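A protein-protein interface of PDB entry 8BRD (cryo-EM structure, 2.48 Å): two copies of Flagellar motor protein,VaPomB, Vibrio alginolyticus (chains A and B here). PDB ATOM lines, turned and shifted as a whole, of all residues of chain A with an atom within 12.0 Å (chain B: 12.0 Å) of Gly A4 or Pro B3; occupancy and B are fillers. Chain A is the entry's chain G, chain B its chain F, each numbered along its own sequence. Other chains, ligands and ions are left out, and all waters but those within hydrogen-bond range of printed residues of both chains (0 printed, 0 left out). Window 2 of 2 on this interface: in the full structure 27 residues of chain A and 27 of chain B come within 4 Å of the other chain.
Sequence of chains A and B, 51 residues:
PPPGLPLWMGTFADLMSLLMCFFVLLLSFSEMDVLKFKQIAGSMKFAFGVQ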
ATOM      1  N   PRO A   1      -3.053  19.672   5.932  1.00  0.00           N
ATOM      2  CA  PRO A   1      -1.724  19.395   5.373  1.00  0.00           C
ATOM      3  C   PRO A   1      -0.597  19.732   6.343  1.00  0.00           C
ATOM      4  O   PRO A   1      -0.655  20.768   7.007  1.00  0.00           O
ATOM      5  CB  PRO A   1      -1.663  20.301   4.139  1.00  0.00           C
ATOM      6  CG  PRO A   1      -3.087  20.563   3.784  1.00  0.00           C
ATOM      7  CD  PRO A   1      -3.821  20.605   5.089  1.00  0.00           C
ATOM      8  N   PRO A   2       0.409  18.868   6.430  1.00  0.00           N
ATOM      9  CA  PRO A   2       1.558  19.150   7.294  1.00  0.00           C
ATOM     10  C   PRO A   2       2.349  20.331   6.767  1.00  0.00           C
ATOM     11  O   PRO A   2       2.644  20.407   5.564  1.00  0.00           O
ATOM     12  CB  PRO A   2       2.375  17.851   7.229  1.00  0.00           C
ATOM     13  CG  PRO A   2       1.992  17.232   5.935  1.00  0.00           C
ATOM     14  CD  PRO A   2       0.554  17.593   5.708  1.00  0.00           C
ATOM     15  N   PRO A   3       2.715  21.272   7.632  1.00  0.00           N
ATOM     16  CA  PRO A   3       3.398  22.478   7.160  1.00  0.00           C
ATOM     17  C   PRO A   3       4.837  22.188   6.768  1.00  0.00           C
ATOM     18  O   PRO A   3       5.338  21.066   6.884  1.00  0.00           O
ATOM     19  CB  PRO A   3       3.332  23.418   8.366  1.00  0.00           C
ATOM     20  CG  PRO A   3       3.280  22.504   9.536  1.00  0.00           C
ATOM     21  CD  PRO A   3       2.519  21.281   9.092  1.00  0.00           C
ATOM     22  N   GLY A   4       5.506  23.235   6.300  1.00  0.00           N
ATOM     23  CA  GLY A   4       6.895  23.124   5.915  1.00  0.00           C
ATOM     24  C   GLY A   4       7.679  24.374   6.247  1.00  0.00           C
ATOM     25  O   GLY A   4       7.402  25.045   7.243  1.00  0.00           O
ATOM     26  N   LEU A   5       8.656  24.699   5.415  1.00  0.00           N
ATOM     27  CA  LEU A   5       9.513  25.854   5.595  1.00  0.00           C
ATOM     28  C   LEU A   5       9.090  26.963   4.642  1.00  0.00           C
ATOM     29  O   LEU A   5       8.497  26.695   3.592  1.00  0.00           O
ATOM     30  CB  LEU A   5      10.978  25.469   5.347  1.00  0.00           C
ATOM     31  CG  LEU A   5      11.454  24.298   6.203  1.00  0.00           C
ATOM     32  CD1 LEU A   5      12.896  23.988   5.903  1.00  0.00           C
ATOM     33  CD2 LEU A   5      11.268  24.589   7.685  1.00  0.00           C
ATOM     34  N   PRO A   6       9.359  28.220   4.985  1.00  0.00           N
ATOM     35  CA  PRO A   6       8.954  29.335   4.115  1.00  0.00           C
ATOM     36  C   PRO A   6       9.622  29.239   2.753  1.00  0.00           C
ATOM     37  O   PRO A   6      10.747  28.736   2.647  1.00  0.00           O
ATOM     38  CB  PRO A   6       9.436  30.571   4.887  1.00  0.00           C
ATOM     39  CG  PRO A   6       9.513  30.128   6.310  1.00  0.00           C
ATOM     40  CD  PRO A   6       9.918  28.690   6.264  1.00  0.00           C
ATOM     41  N   LEU A   7       9.085  29.915   1.812  1.00  0.00           N
ATOM     42  CA  LEU A   7       9.536  29.710   0.452  1.00  0.00           C
ATOM     43  C   LEU A   7      10.844  30.402   0.262  1.00  0.00           C
ATOM     44  O   LEU A   7      11.512  29.988  -0.600  1.00  0.00           O
ATOM     45  CB  LEU A   7       8.408  30.247  -0.391  1.00  0.00           C
ATOM     46  CG  LEU A   7       7.031  29.696  -0.047  1.00  0.00           C
ATOM     47  CD1 LEU A   7       6.023  30.085  -1.107  1.00  0.00           C
ATOM     48  CD2 LEU A   7       7.076  28.187   0.133  1.00  0.00           C
ATOM     49  N   TRP A   8      11.169  31.373   1.070  1.00  0.00           N
ATOM     50  CA  TRP A   8      12.455  32.058   1.000  1.00  0.00           C
ATOM     51  C   TRP A   8      13.583  31.252   1.624  1.00  0.00           C
ATOM     52  O   TRP A   8      14.738  31.680   1.559  1.00  0.00           O
ATOM     53  CB  TRP A   8      12.356  33.432   1.672  1.00  0.00           C
ATOM     54  CG  TRP A   8      11.891  33.403   3.102  1.00  0.00           C
ATOM     55  CD1 TRP A   8      10.645  33.707   3.559  1.00  0.00           C
ATOM     56  CD2 TRP A   8      12.665  33.059   4.262  1.00  0.00           C
ATOM     57  NE1 TRP A   8      10.590  33.569   4.921  1.00  0.00           N
ATOM     58  CE2 TRP A   8      11.817  33.170   5.377  1.00  0.00           C
ATOM     59  CE3 TRP A   8      13.992  32.663   4.462  1.00  0.00           C
ATOM     60  CZ2 TRP A   8      12.247  32.902   6.672  1.00  0.00           C
ATOM     61  CZ3 TRP A   8      14.418  32.396   5.746  1.00  0.00           C
ATOM     62  CH2 TRP A   8      13.548  32.516   6.836  1.00  0.00           C
ATOM     63  N   MET A   9      13.272  30.109   2.232  1.00  0.00           N
ATOM     64  CA  MET A   9      14.280  29.327   2.934  1.00  0.00           C
ATOM     65  C   MET A   9      15.299  28.756   1.953  1.00  0.00           C
ATOM     66  O   MET A   9      16.484  28.614   2.280  1.00  0.00           O
ATOM     67  CB  MET A   9      13.578  28.222   3.727  1.00  0.00           C
ATOM     68  CG  MET A   9      13.681  28.340   5.248  1.00  0.00           C
ATOM     69  SD  MET A   9      15.307  28.730   5.879  1.00  0.00           S
ATOM     70  CE  MET A   9      16.173  27.348   5.177  1.00  0.00           C
ATOM     71  N   GLY A  10      14.858  28.443   0.733  1.00  0.00           N
ATOM     72  CA  GLY A  10      15.790  28.028  -0.301  1.00  0.00           C
ATOM     73  C   GLY A  10      16.754  29.127  -0.695  1.00  0.00           C
ATOM     74  O   GLY A  10      17.950  28.889  -0.868  1.00  0.00           O
ATOM     75  N   PRO B   1      -3.064  26.565   1.468  1.00  0.00           N
ATOM     76  CA  PRO B   1      -1.737  27.159   1.663  1.00  0.00           C
ATOM     77  C   PRO B   1      -0.648  26.409   0.902  1.00  0.00           C
ATOM     78  O   PRO B   1      -0.790  25.210   0.670  1.00  0.00           O
ATOM     79  CB  PRO B   1      -1.518  27.046   3.175  1.00  0.00           C
ATOM     80  CG  PRO B   1      -2.888  26.953   3.753  1.00  0.00           C
ATOM     81  CD  PRO B   1      -3.696  26.194   2.745  1.00  0.00           C
ATOM     82  N   PRO B   2       0.413  27.110   0.510  1.00  0.00           N
ATOM     83  CA  PRO B   2       1.529  26.453  -0.176  1.00  0.00           C
ATOM     84  C   PRO B   2       2.157  25.391   0.708  1.00  0.00           C
ATOM     85  O   PRO B   2       2.220  25.549   1.936  1.00  0.00           O
ATOM     86  CB  PRO B   2       2.507  27.605  -0.449  1.00  0.00           C
ATOM     87  CG  PRO B   2       1.660  28.829  -0.438  1.00  0.00           C
ATOM     88  CD  PRO B   2       0.591  28.569   0.584  1.00  0.00           C
ATOM     89  N   PRO B   3       2.625  24.286   0.118  1.00  0.00           N
ATOM     90  CA  PRO B   3       3.158  23.190   0.941  1.00  0.00           C
ATOM     91  C   PRO B   3       4.397  23.561   1.734  1.00  0.00           C
ATOM     92  O   PRO B   3       4.682  22.910   2.747  1.00  0.00           O
ATOM     93  CB  PRO B   3       3.458  22.091  -0.089  1.00  0.00           C
ATOM     94  CG  PRO B   3       2.681  22.469  -1.312  1.00  0.00           C
ATOM     95  CD  PRO B   3       2.640  23.961  -1.316  1.00  0.00           C
ATOM     96  N   GLY B   4       5.140  24.583   1.319  1.00  0.00           N
ATOM     97  CA  GLY B   4       6.387  24.916   1.973  1.00  0.00           C
ATOM     98  C   GLY B   4       7.551  24.110   1.426  1.00  0.00           C
ATOM     99  O   GLY B   4       7.428  23.326   0.484  1.00  0.00           O
ATOM    100  N   LEU B   5       8.714  24.315   2.043  1.00  0.00           N
ATOM    101  CA  LEU B   5       9.934  23.653   1.607  1.00  0.00           C
ATOM    102  C   LEU B   5      10.286  22.492   2.535  1.00  0.00           C
ATOM    103  O   LEU B   5       9.953  22.515   3.722  1.00  0.00           O
ATOM    104  CB  LEU B   5      11.090  24.647   1.560  1.00  0.00           C
ATOM    105  CG  LEU B   5      10.949  25.780   0.544  1.00  0.00           C
ATOM    106  CD1 LEU B   5      12.240  26.558   0.425  1.00  0.00           C
ATOM    107  CD2 LEU B   5      10.533  25.238  -0.811  1.00  0.00           C
ATOM    108  N   PRO B   6      10.948  21.463   2.011  1.00  0.00           N
ATOM    109  CA  PRO B   6      11.206  20.262   2.812  1.00  0.00           C
ATOM    110  C   PRO B   6      12.241  20.501   3.903  1.00  0.00           C
ATOM    111  O   PRO B   6      13.057  21.424   3.841  1.00  0.00           O
ATOM    112  CB  PRO B   6      11.713  19.246   1.784  1.00  0.00           C
ATOM    113  CG  PRO B   6      11.427  19.847   0.444  1.00  0.00           C
ATOM    114  CD  PRO B   6      11.436  21.313   0.631  1.00  0.00           C
ATOM    115  N   LEU B   7      12.200  19.624   4.911  1.00  0.00           N
ATOM    116  CA  LEU B   7      13.034  19.782   6.098  1.00  0.00           C
ATOM    117  C   LEU B   7      14.523  19.705   5.779  1.00  0.00           C
ATOM    118  O   LEU B   7      15.339  20.324   6.479  1.00  0.00           O
ATOM    119  CB  LEU B   7      12.661  18.720   7.132  1.00  0.00           C
ATOM    120  CG  LEU B   7      13.157  18.931   8.564  1.00  0.00           C
ATOM    121  CD1 LEU B   7      12.732  20.298   9.084  1.00  0.00           C
ATOM    122  CD2 LEU B   7      12.661  17.818   9.476  1.00  0.00           C
ATOM    123  N   TRP B   8      14.900  18.949   4.748  1.00  0.00           N
ATOM    124  CA  TRP B   8      16.309  18.870   4.387  1.00  0.00           C
ATOM    125  C   TRP B   8      16.850  20.236   3.996  1.00  0.00           C
ATOM    126  O   TRP B   8      18.035  20.503   4.182  1.00  0.00           O
ATOM    127  CB  TRP B   8      16.528  17.858   3.253  1.00  0.00           C
ATOM    128  CG  TRP B   8      16.000  18.303   1.925  1.00  0.00           C
ATOM    129  CD1 TRP B   8      14.815  17.955   1.364  1.00  0.00           C
ATOM    130  CD2 TRP B   8      16.638  19.190   0.997  1.00  0.00           C
ATOM    131  NE1 TRP B   8      14.667  18.567   0.146  1.00  0.00           N
ATOM    132  CE2 TRP B   8      15.773  19.333  -0.100  1.00  0.00           C
ATOM    133  CE3 TRP B   8      17.852  19.880   0.991  1.00  0.00           C
ATOM    134  CZ2 TRP B   8      16.082  20.137  -1.189  1.00  0.00           C
ATOM    135  CZ3 TRP B   8      18.156  20.672  -0.089  1.00  0.00           C
ATOM    136  CH2 TRP B   8      17.278  20.793  -1.167  1.00  0.00           C
ATOM    137  N   MET B   9      16.001  21.113   3.456  1.00  0.00           N
ATOM    138  CA  MET B   9      16.452  22.459   3.112  1.00  0.00           C
ATOM    139  C   MET B   9      16.767  23.272   4.362  1.00  0.00           C
ATOM    140  O   MET B   9      17.728  24.052   4.381  1.00  0.00           O
ATOM    141  CB  MET B   9      15.400  23.159   2.257  1.00  0.00           C
ATOM    142  CG  MET B   9      15.825  24.520   1.739  1.00  0.00           C
ATOM    143  SD  MET B   9      16.790  24.403   0.225  1.00  0.00           S
ATOM    144  CE  MET B   9      15.486  24.472  -0.999  1.00  0.00           C
ATOM    145  N   GLY B  10      15.972  23.104   5.419  1.00  0.00           N
ATOM    146  CA  GLY B  10      16.309  23.726   6.686  1.00  0.00           C
ATOM    147  C   GLY B  10      17.603  23.188   7.261  1.00  0.00           C
ATOM    148  O   GLY B  10      18.436  23.949   7.758  1.00  0.00           O
ATOM    149  N   THR B  11      17.793  21.870   7.189  1.00  0.00           N
ATOM    150  CA  THR B  11      19.064  21.287   7.610  1.00  0.00           C
ATOM    151  C   THR B  11      20.224  21.856   6.801  1.00  0.00           C
ATOM    152  O   THR B  11      21.286  22.167   7.352  1.00  0.00           O
ATOM    153  CB  THR B  11      19.008  19.765   7.470  1.00  0.00           C
ATOM    154  OG1 THR B  11      17.918  19.253   8.245  1.00  0.00           O
ATOM    155  CG2 THR B  11      20.302  19.132   7.945  1.00  0.00           C
ATOM    156  N   ASP B  14      20.955  25.452   7.947  1.00  0.00           N
ATOM    157  CA  ASP B  14      21.641  25.439   9.236  1.00  0.00           C
ATOM    158  C   ASP B  14      23.095  25.022   9.083  1.00  0.00           C
ATOM    159  O   ASP B  14      23.990  25.638   9.674  1.00  0.00           O
ATOM    160  CB  ASP B  14      20.924  24.521  10.222  1.00  0.00           C
ATOM    161  CG  ASP B  14      19.454  24.832  10.343  1.00  0.00           C
ATOM    162  OD1 ASP B  14      18.994  25.792   9.695  1.00  0.00           O
ATOM    163  OD2 ASP B  14      18.752  24.117  11.089  1.00  0.00           O
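O of Leu A5 is in hydrogen-bond range of N of Leu B5.
The side-chain carboxylate (OD1) of Asp B14 lies close to the backbone carbonyl oxygen (O) of Gly B10, at 2.7 Å.
Among the printed residues, merely in contact across the chains: Gly A4 with Pro B3 (3.7 Å), Gly A4 with Leu B5 (3.8 Å), Leu A5 with Gly B4 (3.2 Å), Leu A5 with Pro B6 (3.3 Å), Leu A5 with Gly B10 (3.2 Å), Pro A6 with Leu B5 (3.5 Å), Leu A7 with Gly B4 (3.8 Å), Leu A7 with Leu B5 (3.7 Å), Met A9 with Leu B5 (3.9 Å), Met A9 with Met B9 (3.7 Å), Met A9 with Gly B10 (3.9 Å), Gly A10 with Leu B5 (3.2 Å) and Gly A10 with Met B9 (3.6 Å).
Pro A3 touches none of the printed residues of chain B. Of chain B, only Pro B3 and Leu B5 come within 4 Å of Gly A4. Of the printed residues of chain B, Leu A5 touches Gly B4 (3.2 Å), Leu B5 (2.8 Å), Pro B6 (3.3 Å) and Gly B10 (3.2 Å). Pro A6 touches just one residue of chain B: Leu B5 (3.5 Å). Printed residues of chain B within 4 Å of Met A9: Leu B5, Met B9 and Gly B10. No residue of chain A comes within 4 Å of Pro B1. Of the printed residues of chain A, Pro B3 touches Gly A4 (3.7 Å). Leu B5 touches just these residues of chain A: Gly A4 (3.8 Å), Leu A5 (2.8 Å), Pro A6 (3.5 Å), Leu A7 (3.7 Å), Met A9 (3.9 Å) and Gly A10 (3.2 Å). Printed residues of chain A within 4 Å of Met B9: Met A9 and Gly A10. Asp B14 touches none of the printed residues of chain A. The nearest residue of chain A that does not touch Pro B3 is Pro A3 (4.1 Å). The nearest printed residue of chain A that does not touch Gly B10 is Gly A10 (7.2 Å).
Of the 12 printed residues of chain B, 6 touch a printed residue of chain A. Printed residues of chain A that touch a printed residue of chain B: Gly A4, Leu A5, Pro A6, Leu A7, Met A9 and Gly A10. Along chain A the printed residues that touch a printed residue of chain B span positions 4 to 10. Among the printed residues, 14 pairs touch across the chains. Among the printed residues, no Asp or Glu carboxylate lies within 4 Å of a Lys or Arg side-chain nitrogen of the other chain.
Gly A4 touches Pro B3, but with the chains exchanged Pro A3 does not touch Gly B4 (5.7 Å). Gly A4 touches Leu B5, and with the chains exchanged Leu A5 touches Gly B4. Leu B5 touches its own counterpart, Leu A5. Met A9 touches Gly B10, and with the chains exchanged Gly A10 touches Met B9. 10 positions are printed for both chains.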
